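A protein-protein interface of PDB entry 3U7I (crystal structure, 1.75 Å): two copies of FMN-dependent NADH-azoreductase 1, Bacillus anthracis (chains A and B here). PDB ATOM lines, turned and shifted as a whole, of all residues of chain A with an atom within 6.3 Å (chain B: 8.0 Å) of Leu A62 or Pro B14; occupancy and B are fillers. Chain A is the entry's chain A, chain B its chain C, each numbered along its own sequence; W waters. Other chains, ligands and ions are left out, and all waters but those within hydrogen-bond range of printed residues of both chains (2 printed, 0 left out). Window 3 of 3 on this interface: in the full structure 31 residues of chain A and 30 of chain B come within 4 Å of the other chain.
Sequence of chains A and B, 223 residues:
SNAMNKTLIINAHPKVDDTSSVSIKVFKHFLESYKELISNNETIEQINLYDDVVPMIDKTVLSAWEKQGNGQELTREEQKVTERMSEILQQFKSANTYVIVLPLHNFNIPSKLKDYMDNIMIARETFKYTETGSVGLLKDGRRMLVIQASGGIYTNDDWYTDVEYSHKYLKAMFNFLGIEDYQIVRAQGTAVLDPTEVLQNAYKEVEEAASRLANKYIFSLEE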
ATOM      1  N   ILE A  57       0.000 -27.634   6.043  1.00  0.00           N
ATOM      2  CA  ILE A  57       0.064 -26.397   6.819  1.00  0.00           C
ATOM      3  C   ILE A  57      -1.333 -25.987   7.281  1.00  0.00           C
ATOM      4  O   ILE A  57      -2.206 -25.666   6.469  1.00  0.00           O
ATOM      5  CB  ILE A  57       0.721 -25.246   6.030  1.00  0.00           C
ATOM      6  CG1 ILE A  57       2.175 -25.587   5.698  1.00  0.00           C
ATOM      7  CG2 ILE A  57       0.663 -23.949   6.830  1.00  0.00           C
ATOM      8  CD1 ILE A  57       2.826 -24.577   4.787  1.00  0.00           C
ATOM      9  N   ASP A  58      -1.537 -26.023   8.594  1.00  0.00           N
ATOM     10  CA  ASP A  58      -2.797 -25.608   9.200  1.00  0.00           C
ATOM     11  C   ASP A  58      -2.518 -24.623  10.335  1.00  0.00           C
ATOM     12  O   ASP A  58      -1.375 -24.195  10.513  1.00  0.00           O
ATOM     13  CB  ASP A  58      -3.627 -26.822   9.681  1.00  0.00           C
ATOM     14  CG  ASP A  58      -2.925 -27.650  10.765  1.00  0.00           C
ATOM     15  OD1 ASP A  58      -1.898 -27.208  11.319  1.00  0.00           O
ATOM     16  OD2 ASP A  58      -3.414 -28.755  11.079  1.00  0.00           O
ATOM     17  N   LYS A  59      -3.559 -24.263  11.086  1.00  0.00           N
ATOM     18  CA  LYS A  59      -3.445 -23.345  12.225  1.00  0.00           C
ATOM     19  C   LYS A  59      -2.361 -23.767  13.223  1.00  0.00           C
ATOM     20  O   LYS A  59      -1.643 -22.922  13.757  1.00  0.00           O
ATOM     21  CB  LYS A  59      -4.788 -23.233  12.954  1.00  0.00           C
ATOM     22  CG  LYS A  59      -5.838 -22.406  12.232  1.00  0.00           C
ATOM     23  CD  LYS A  59      -7.190 -22.453  12.943  1.00  0.00           C
ATOM     24  CE  LYS A  59      -8.105 -21.324  12.465  1.00  0.00           C
ATOM     25  NZ  LYS A  59      -9.535 -21.497  12.870  1.00  0.00           N
ATOM     26  N   THR A  60      -2.252 -25.071  13.463  1.00  0.00           N
ATOM     27  CA  THR A  60      -1.318 -25.601  14.456  1.00  0.00           C
ATOM     28  C   THR A  60       0.126 -25.484  13.982  1.00  0.00           C
ATOM     29  O   THR A  60       1.005 -25.106  14.755  1.00  0.00           O
ATOM     30  CB  THR A  60      -1.637 -27.074  14.831  1.00  0.00           C
ATOM     31  OG1 THR A  60      -2.999 -27.179  15.273  1.00  0.00           O
ATOM     32  CG2 THR A  60      -0.713 -27.561  15.942  1.00  0.00           C
ATOM     33  N   VAL A  61       0.365 -25.800  12.708  1.00  0.00           N
ATOM     34  CA  VAL A  61       1.696 -25.669  12.112  1.00  0.00           C
ATOM     35  C   VAL A  61       2.145 -24.197  12.078  1.00  0.00           C
ATOM     36  O   VAL A  61       3.297 -23.882  12.378  1.00  0.00           O
ATOM     37  CB  VAL A  61       1.750 -26.288  10.682  1.00  0.00           C
ATOM     38  CG1 VAL A  61       3.039 -25.914   9.960  1.00  0.00           C
ATOM     39  CG2 VAL A  61       1.571 -27.798  10.742  1.00  0.00           C
ATOM     40  N   LEU A  62       1.235 -23.296  11.720  1.00  0.00           N
ATOM     41  CA  LEU A  62       1.579 -21.878  11.656  1.00  0.00           C
ATOM     42  C   LEU A  62       1.912 -21.351  13.053  1.00  0.00           C
ATOM     43  O   LEU A  62       2.880 -20.613  13.234  1.00  0.00           O
ATOM     44  CB  LEU A  62       0.456 -21.069  10.987  1.00  0.00           C
ATOM     45  CG  LEU A  62       0.258 -21.350   9.489  1.00  0.00           C
ATOM     46  CD1 LEU A  62      -1.035 -20.706   8.960  1.00  0.00           C
ATOM     47  CD2 LEU A  62       1.480 -20.914   8.673  1.00  0.00           C
ATOM     48  N   SER A  63       1.113 -21.744  14.041  1.00  0.00           N
ATOM     49  CA  SER A  63       1.356 -21.360  15.431  1.00  0.00           C
ATOM     50  C   SER A  63       2.733 -21.849  15.873  1.00  0.00           C
ATOM     51  O   SER A  63       3.492 -21.111  16.500  1.00  0.00           O
ATOM     52  CB  SER A  63       0.276 -21.950  16.338  1.00  0.00           C
ATOM     53  OG  SER A  63       0.576 -21.736  17.707  1.00  0.00           O
ATOM     54  N   ALA A  64       3.048 -23.098  15.537  1.00  0.00           N
ATOM     55  CA  ALA A  64       4.327 -23.708  15.909  1.00  0.00           C
ATOM     56  C   ALA A  64       5.508 -22.950  15.314  1.00  0.00           C
ATOM     57  O   ALA A  64       6.504 -22.705  15.993  1.00  0.00           O
ATOM     58  CB  ALA A  64       4.366 -25.172  15.481  1.00  0.00           C
ATOM     59  N   TRP A  65       5.386 -22.587  14.039  1.00  0.00           N
ATOM     60  CA  TRP A  65       6.438 -21.856  13.331  1.00  0.00           C
ATOM     61  C   TRP A  65       6.650 -20.450  13.888  1.00  0.00           C
ATOM     62  O   TRP A  65       7.784 -19.981  13.996  1.00  0.00           O
ATOM     63  CB  TRP A  65       6.138 -21.803  11.831  1.00  0.00           C
ATOM     64  CG  TRP A  65       6.395 -23.105  11.125  1.00  0.00           C
ATOM     65  CD1 TRP A  65       7.028 -24.211  11.635  1.00  0.00           C
ATOM     66  CD2 TRP A  65       6.029 -23.437   9.777  1.00  0.00           C
ATOM     67  NE1 TRP A  65       7.076 -25.208  10.684  1.00  0.00           N
ATOM     68  CE2 TRP A  65       6.473 -24.760   9.538  1.00  0.00           C
ATOM     69  CE3 TRP A  65       5.372 -22.748   8.750  1.00  0.00           C
ATOM     70  CZ2 TRP A  65       6.277 -25.402   8.312  1.00  0.00           C
ATOM     71  CZ3 TRP A  65       5.175 -23.392   7.532  1.00  0.00           C
ATOM     72  CH2 TRP A  65       5.626 -24.705   7.326  1.00  0.00           C
ATOM     73  N   GLU A  66       5.557 -19.776  14.237  1.00  0.00           N
ATOM     74  CA  GLU A  66       5.649 -18.474  14.893  1.00  0.00           C
ATOM     75  C   GLU A  66       6.409 -18.592  16.214  1.00  0.00           C
ATOM     76  O   GLU A  66       7.329 -17.822  16.469  1.00  0.00           O
ATOM     77  CB  GLU A  66       4.260 -17.882  15.135  1.00  0.00           C
ATOM     78  CG  GLU A  66       3.516 -17.527  13.857  1.00  0.00           C
ATOM     79  CD  GLU A  66       2.068 -17.143  14.110  1.00  0.00           C
ATOM     80  OE1 GLU A  66       1.750 -16.784  15.267  1.00  0.00           O
ATOM     81  OE2 GLU A  66       1.254 -17.208  13.158  1.00  0.00           O
ATOM     82  N   LYS A  67       6.015 -19.564  17.040  1.00  0.00           N
ATOM     83  CA  LYS A  67       6.640 -19.793  18.345  1.00  0.00           C
ATOM     84  C   LYS A  67       8.105 -20.191  18.210  1.00  0.00           C
ATOM     85  O   LYS A  67       8.934 -19.828  19.052  1.00  0.00           O
ATOM     86  CB  LYS A  67       5.890 -20.868  19.141  1.00  0.00           C
ATOM     87  CG  LYS A  67       4.484 -20.487  19.562  1.00  0.00           C
ATOM     88  CD  LYS A  67       3.820 -21.619  20.324  1.00  0.00           C
ATOM     89  CE  LYS A  67       2.412 -21.247  20.741  1.00  0.00           C
ATOM     90  NZ  LYS A  67       1.772 -22.351  21.492  1.00  0.00           N
ATOM     91  N   ASN B  11     -12.598 -19.111   0.834  1.00  0.00           N
ATOM     92  CA  ASN B  11     -11.512 -18.736   1.727  1.00  0.00           C
ATOM     93  C   ASN B  11     -10.465 -19.851   1.848  1.00  0.00           C
ATOM     94  O   ASN B  11     -10.701 -20.867   2.507  1.00  0.00           O
ATOM     95  CB  ASN B  11     -12.086 -18.374   3.097  1.00  0.00           C
ATOM     96  CG  ASN B  11     -11.016 -18.017   4.106  1.00  0.00           C
ATOM     97  OD1 ASN B  11      -9.822 -17.970   3.787  1.00  0.00           O
ATOM     98  ND2 ASN B  11     -11.445 -17.742   5.338  1.00  0.00           N
ATOM     99  N   ALA B  12      -9.314 -19.658   1.214  1.00  0.00           N
ATOM    100  CA  ALA B  12      -8.276 -20.698   1.194  1.00  0.00           C
ATOM    101  C   ALA B  12      -7.168 -20.486   2.248  1.00  0.00           C
ATOM    102  O   ALA B  12      -6.074 -21.050   2.136  1.00  0.00           O
ATOM    103  CB  ALA B  12      -7.673 -20.820  -0.204  1.00  0.00           C
ATOM    104  N   HIS B  13      -7.451 -19.677   3.265  1.00  0.00           N
ATOM    105  CA  HIS B  13      -6.462 -19.378   4.294  1.00  0.00           C
ATOM    106  C   HIS B  13      -6.533 -20.381   5.447  1.00  0.00           C
ATOM    107  O   HIS B  13      -7.577 -20.545   6.052  1.00  0.00           O
ATOM    108  CB  HIS B  13      -6.655 -17.960   4.837  1.00  0.00           C
ATOM    109  CG  HIS B  13      -5.399 -17.359   5.389  1.00  0.00           C
ATOM    110  ND1 HIS B  13      -4.691 -17.937   6.421  1.00  0.00           N
ATOM    111  CD2 HIS B  13      -4.712 -16.246   5.038  1.00  0.00           C
ATOM    112  CE1 HIS B  13      -3.626 -17.202   6.689  1.00  0.00           C
ATOM    113  NE2 HIS B  13      -3.614 -16.171   5.864  1.00  0.00           N
ATOM    114  N   PRO B  14      -5.411 -21.056   5.753  1.00  0.00           N
ATOM    115  CA  PRO B  14      -5.378 -22.014   6.866  1.00  0.00           C
ATOM    116  C   PRO B  14      -5.849 -21.433   8.216  1.00  0.00           C
ATOM    117  O   PRO B  14      -6.325 -22.181   9.071  1.00  0.00           O
ATOM    118  CB  PRO B  14      -3.892 -22.408   6.938  1.00  0.00           C
ATOM    119  CG  PRO B  14      -3.398 -22.236   5.525  1.00  0.00           C
ATOM    120  CD  PRO B  14      -4.149 -21.035   4.990  1.00  0.00           C
ATOM    121  N   LYS B  15      -5.715 -20.124   8.414  1.00  0.00           N
ATOM    122  CA  LYS B  15      -6.132 -19.514   9.675  1.00  0.00           C
ATOM    123  C   LYS B  15      -7.599 -19.081   9.659  1.00  0.00           C
ATOM    124  O   LYS B  15      -8.098 -18.514  10.636  1.00  0.00           O
ATOM    125  CB  LYS B  15      -5.242 -18.323  10.030  1.00  0.00           C
ATOM    126  CG  LYS B  15      -3.805 -18.677  10.365  1.00  0.00           C
ATOM    127  CD  LYS B  15      -3.176 -17.531  11.112  1.00  0.00           C
ATOM    128  CE  LYS B  15      -1.720 -17.780  11.379  1.00  0.00           C
ATOM    129  NZ  LYS B  15      -1.227 -16.838  12.423  1.00  0.00           N
ATOM    130  N   VAL B  16      -8.270 -19.335   8.536  1.00  0.00           N
ATOM    131  CA  VAL B  16      -9.713 -19.118   8.392  1.00  0.00           C
ATOM    132  C   VAL B  16     -10.160 -17.658   8.596  1.00  0.00           C
ATOM    133  O   VAL B  16     -10.404 -16.937   7.631  1.00  0.00           O
ATOM    134  CB  VAL B  16     -10.522 -20.071   9.319  1.00  0.00           C
ATOM    135  CG1 VAL B  16     -12.009 -20.033   8.972  1.00  0.00           C
ATOM    136  CG2 VAL B  16      -9.982 -21.496   9.217  1.00  0.00           C
ATOM    137  N   ASP B  17     -10.264 -17.224   9.849  1.00  0.00           N
ATOM    138  CA  ASP B  17     -10.866 -15.920  10.147  1.00  0.00           C
ATOM    139  C   ASP B  17      -9.950 -14.954  10.905  1.00  0.00           C
ATOM    140  O   ASP B  17     -10.296 -13.779  11.079  1.00  0.00           O
ATOM    141  CB  ASP B  17     -12.185 -16.104  10.905  1.00  0.00           C
ATOM    142  CG  ASP B  17     -12.026 -16.958  12.158  1.00  0.00           C
ATOM    143  OD1 ASP B  17     -10.957 -17.598  12.322  1.00  0.00           O
ATOM    144  OD2 ASP B  17     -12.975 -16.995  12.975  1.00  0.00           O
ATOM    145  N   ASP B  18      -8.796 -15.449  11.349  1.00  0.00           N
ATOM    146  CA  ASP B  18      -7.815 -14.628  12.056  1.00  0.00           C
ATOM    147  C   ASP B  18      -7.578 -13.284  11.362  1.00  0.00           C
ATOM    148  O   ASP B  18      -7.147 -13.232  10.210  1.00  0.00           O
ATOM    149  CB  ASP B  18      -6.496 -15.387  12.213  1.00  0.00           C
ATOM    150  CG  ASP B  18      -5.518 -14.675  13.128  1.00  0.00           C
ATOM    151  OD1 ASP B  18      -4.738 -13.835  12.632  1.00  0.00           O
ATOM    152  OD2 ASP B  18      -5.522 -14.959  14.347  1.00  0.00           O
ATOM    153  N   SER B  21      -4.146 -11.672   9.476  1.00  0.00           N
ATOM    154  CA  SER B  21      -3.682 -12.131   8.167  1.00  0.00           C
ATOM    155  C   SER B  21      -3.888 -11.048   7.124  1.00  0.00           C
ATOM    156  O   SER B  21      -5.005 -10.544   6.971  1.00  0.00           O
ATOM    157  CB  SER B  21      -4.440 -13.387   7.735  1.00  0.00           C
ATOM    158  OG  SER B  21      -4.226 -14.448   8.644  1.00  0.00           O
ATOM    159  N   SER B  23      -4.121 -11.072   3.811  1.00  0.00           N
ATOM    160  CA  SER B  23      -5.184 -11.399   2.861  1.00  0.00           C
ATOM    161  C   SER B  23      -6.582 -11.355   3.504  1.00  0.00           C
ATOM    162  O   SER B  23      -7.557 -10.972   2.864  1.00  0.00           O
ATOM    163  CB  SER B  23      -4.931 -12.752   2.186  1.00  0.00           C
ATOM    164  OG  SER B  23      -4.927 -13.813   3.123  1.00  0.00           O
ATOM    165  N   ILE B  24      -6.676 -11.739   4.771  1.00  0.00           N
ATOM    166  CA  ILE B  24      -7.951 -11.669   5.486  1.00  0.00           C
ATOM    167  C   ILE B  24      -8.365 -10.213   5.778  1.00  0.00           C
ATOM    168  O   ILE B  24      -9.530  -9.862   5.612  1.00  0.00           O
ATOM    169  CB  ILE B  24      -7.932 -12.530   6.776  1.00  0.00           C
ATOM    170  CG1 ILE B  24      -7.731 -14.013   6.419  1.00  0.00           C
ATOM    171  CG2 ILE B  24      -9.214 -12.337   7.567  1.00  0.00           C
ATOM    172  CD1 ILE B  24      -7.390 -14.922   7.601  1.00  0.00           C
ATOM    173  N   LEU B  49     -12.142 -23.358   3.390  1.00  0.00           N
ATOM    174  CA  LEU B  49     -11.471 -24.575   2.932  1.00  0.00           C
ATOM    175  C   LEU B  49     -10.667 -25.271   4.023  1.00  0.00           C
ATOM    176  O   LEU B  49     -10.391 -26.461   3.913  1.00  0.00           O
ATOM    177  CB  LEU B  49     -10.575 -24.298   1.720  1.00  0.00           C
ATOM    178  CG  LEU B  49     -11.264 -23.647   0.515  1.00  0.00           C
ATOM    179  CD1 LEU B  49     -10.327 -23.595  -0.697  1.00  0.00           C
ATOM    180  CD2 LEU B  49     -12.548 -24.377   0.172  1.00  0.00           C
ATOM    181  N   TYR B  50     -10.300 -24.545   5.078  1.00  0.00           N
ATOM    182  CA  TYR B  50      -9.527 -25.142   6.169  1.00  0.00           C
ATOM    183  C   TYR B  50     -10.358 -25.335   7.441  1.00  0.00           C
ATOM    184  O   TYR B  50      -9.817 -25.578   8.522  1.00  0.00           O
ATOM    185  CB  TYR B  50      -8.251 -24.329   6.439  1.00  0.00           C
ATOM    186  CG  TYR B  50      -7.197 -24.581   5.389  1.00  0.00           C
ATOM    187  CD1 TYR B  50      -7.231 -23.928   4.153  1.00  0.00           C
ATOM    188  CD2 TYR B  50      -6.191 -25.509   5.615  1.00  0.00           C
ATOM    189  CE1 TYR B  50      -6.269 -24.189   3.184  1.00  0.00           C
ATOM    190  CE2 TYR B  50      -5.242 -25.779   4.665  1.00  0.00           C
ATOM    191  CZ  TYR B  50      -5.275 -25.122   3.454  1.00  0.00           C
ATOM    192  OH  TYR B  50      -4.298 -25.433   2.534  1.00  0.00           O
ATOM    193  N   ASP B  51     -11.680 -25.239   7.293  1.00  0.00           N
ATOM    194  CA  ASP B  51     -12.593 -25.482   8.407  1.00  0.00           C
ATOM    195  C   ASP B  51     -13.783 -26.344   7.984  1.00  0.00           C
ATOM    196  O   ASP B  51     -14.141 -27.303   8.675  1.00  0.00           O
ATOM    197  CB  ASP B  51     -13.084 -24.158   9.006  1.00  0.00           C
ATOM    198  CG  ASP B  51     -13.771 -24.340  10.347  1.00  0.00           C
ATOM    199  OD1 ASP B  51     -13.144 -24.906  11.276  1.00  0.00           O
ATOM    200  OD2 ASP B  51     -14.943 -23.921  10.463  1.00  0.00           O
ATOM    201  N   VAL B 101      -9.721 -16.057  -1.548  1.00  0.00           N
ATOM    202  CA  VAL B 101      -8.760 -15.475  -0.610  1.00  0.00           C
ATOM    203  C   VAL B 101      -7.672 -16.506  -0.276  1.00  0.00           C
ATOM    204  O   VAL B 101      -7.966 -17.607   0.189  1.00  0.00           O
ATOM    205  CB  VAL B 101      -9.460 -14.989   0.695  1.00  0.00           C
ATOM    206  CG1 VAL B 101      -8.511 -14.145   1.561  1.00  0.00           C
ATOM    207  CG2 VAL B 101     -10.747 -14.209   0.354  1.00  0.00           C
ATOM    208  N   LEU B 102      -6.417 -16.155  -0.521  1.00  0.00           N
ATOM    209  CA  LEU B 102      -5.330 -17.084  -0.232  1.00  0.00           C
ATOM    210  C   LEU B 102      -4.039 -16.379   0.114  1.00  0.00           C
ATOM    211  O   LEU B 102      -3.765 -15.281  -0.391  1.00  0.00           O
ATOM    212  CB  LEU B 102      -5.070 -18.010  -1.423  1.00  0.00           C
ATOM    213  CG  LEU B 102      -4.399 -17.379  -2.647  1.00  0.00           C
ATOM    214  CD1 LEU B 102      -3.764 -18.449  -3.537  1.00  0.00           C
ATOM    215  CD2 LEU B 102      -5.414 -16.540  -3.419  1.00  0.00           C
ATOM    216  N   PRO B 103      -3.249 -17.004   1.003  1.00  0.00           N
ATOM    217  CA  PRO B 103      -1.831 -16.675   1.149  1.00  0.00           C
ATOM    218  C   PRO B 103      -1.050 -17.485   0.120  1.00  0.00           C
ATOM    219  O   PRO B 103      -1.357 -18.660  -0.091  1.00  0.00           O
ATOM    220  CB  PRO B 103      -1.506 -17.155   2.564  1.00  0.00           C
ATOM    221  CG  PRO B 103      -2.433 -18.282   2.799  1.00  0.00           C
ATOM    222  CD  PRO B 103      -3.699 -17.967   2.026  1.00  0.00           C
ATOM    223  N   HIS B 105       1.957 -19.507  -0.594  1.00  0.00           N
ATOM    224  CA  HIS B 105       3.083 -20.202   0.009  1.00  0.00           C
ATOM    225  C   HIS B 105       3.626 -21.217  -0.975  1.00  0.00           C
ATOM    226  O   HIS B 105       2.876 -22.038  -1.508  1.00  0.00           O
ATOM    227  CB  HIS B 105       2.690 -20.894   1.314  1.00  0.00           C
ATOM    228  CG  HIS B 105       3.869 -21.340   2.128  1.00  0.00           C
ATOM    229  ND1 HIS B 105       4.945 -20.517   2.395  1.00  0.00           N
ATOM    230  CD2 HIS B 105       4.148 -22.526   2.721  1.00  0.00           C
ATOM    231  CE1 HIS B 105       5.832 -21.176   3.123  1.00  0.00           C
ATOM    232  NE2 HIS B 105       5.371 -22.395   3.337  1.00  0.00           N
ATOM    233  N   PRO B 110      -2.907 -23.181  -2.211  1.00  0.00           N
ATOM    234  CA  PRO B 110      -2.950 -24.036  -1.021  1.00  0.00           C
ATOM    235  C   PRO B 110      -3.489 -25.429  -1.352  1.00  0.00           C
ATOM    236  O   PRO B 110      -4.379 -25.570  -2.188  1.00  0.00           O
ATOM    237  CB  PRO B 110      -3.923 -23.292  -0.100  1.00  0.00           C
ATOM    238  CG  PRO B 110      -3.764 -21.867  -0.467  1.00  0.00           C
ATOM    239  CD  PRO B 110      -3.554 -21.873  -1.968  1.00  0.00           C
ATOM    240  N   SER B 111      -2.961 -26.451  -0.684  1.00  0.00           N
ATOM    241  CA  SER B 111      -3.421 -27.822  -0.915  1.00  0.00           C
ATOM    242  C   SER B 111      -4.943 -27.955  -0.876  1.00  0.00           C
ATOM    243  O   SER B 111      -5.526 -28.654  -1.706  1.00  0.00           O
ATOM    244  CB  SER B 111      -2.784 -28.785   0.080  1.00  0.00           C
ATOM    245  OG  SER B 111      -3.049 -28.382   1.408  1.00  0.00           O
ATOM    246  N   LYS B 112      -5.591 -27.296   0.083  1.00  0.00           N
ATOM    247  CA  LYS B 112      -7.050 -27.407   0.179  1.00  0.00           C
ATOM    248  C   LYS B 112      -7.772 -26.702  -0.977  1.00  0.00           C
ATOM    249  O   LYS B 112      -8.893 -27.062  -1.311  1.00  0.00           O
ATOM    250  CB  LYS B 112      -7.586 -26.957   1.552  1.00  0.00           C
ATOM    251  CG  LYS B 112      -7.186 -27.857   2.724  1.00  0.00           C
ATOM    252  CD  LYS B 112      -7.516 -29.339   2.501  1.00  0.00           C
ATOM    253  CE  LYS B 112      -9.022 -29.603   2.355  1.00  0.00           C
ATOM    254  NZ  LYS B 112      -9.338 -31.084   2.289  1.00  0.00           N
HETATM  255  O   HOH W   1      -2.241 -26.045   3.687  1.00  0.00           O
HETATM  256  O   HOH W   2      -6.120 -24.660   9.791  1.00  0.00           O
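Printed residues of chain B that touch a printed residue of chain A: Pro B14, Lys B15, Val B16, Tyr B50 and His B105. Printed residues of chain A that touch a printed residue of chain B: Ile A57, Lys A59, Leu A62 and Glu A66. Hydrophobic or aromatic side chains of chain A within 4 Å of the printed part of chain B: Ile A57 and Leu A62. Among the printed residues, 9 pairs touch across the chains.
Of chain A, only Ile A57 (3.7 Å), Lys A59 (3.2 Å) and Leu A62 (3.9 Å) come within 4 Å of Pro B14. Printed residues of chain B within 4 Å of Lys A59: Pro B14 (3.2 Å), Lys B15 (3.4 Å) and Val B16 (3.7 Å). Printed residues of chain A within 4 Å of Tyr B50: Ile A57. Printed residues of chain A within 4 Å of Lys B15: Lys A59 (3.4 Å), Leu A62 (3.7 Å) and Glu A66 (2.6 Å). Of the printed residues of chain A, His B105 touches Ile A57 (3.2 Å). Of the printed residues of chain B, Glu A66 touches Lys B15 (2.6 Å). The nearest residue of chain A that does not touch Pro B14 is Asp A58 (4.1 Å). The nearest printed residue of chain A that does not touch Lys B15 is Ser A63 (5.6 Å).
The side-chain hydroxyl of Tyr B50 lies within hydrogen-bond range of the side-chain hydroxyl of Ser B111, 3.4 Å away. The side-chain hydroxyl (OH) of Tyr B50 sits at hydrogen-bond distance from the backbone NH (N) of Lys B112 (3.3 Å). The backbone carbonyl oxygen of Val B16 sits at hydrogen-bond distance from the side-chain amide nitrogen of Asn B11 (2.6 Å). ND1 of His B13 sits close to N of Lys B15.
No position is printed for both chains. Of the 9 pairs that touch across the chains among the printed residues, none has its exchanged pair printed and touching as well.
OE2 of Glu A66 lies within salt-bridge range of NZ of Lys B15.
O of Ile A57 touches CB of Pro B14 (3.7 Å). O of Ile A57 touches CE2 of Tyr B50, 3.5 Å away. CD1 of Ile A57 touches CD2 of His B105, 3.2 Å away. Lys A59 touches Pro B14 (CG to O, 3.2 Å). Lys B15 touches Lys A59. Val B16 touches Lys A59 (CG2 to NZ, 3.7 Å). Leu A62 touches Pro B14. Lys B15 touches Leu A62.
Water W1 lies within hydrogen-bond range of the side-chain hydroxyl (OH) of Tyr B50, the backbone carbonyl oxygen (O) of Ile A57 and the side-chain hydroxyl (OG) of Ser B111. Water W2 lies within hydrogen-bond range of O of Pro B14 (2.6 Å) and N of Lys A59 (2.9 Å).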
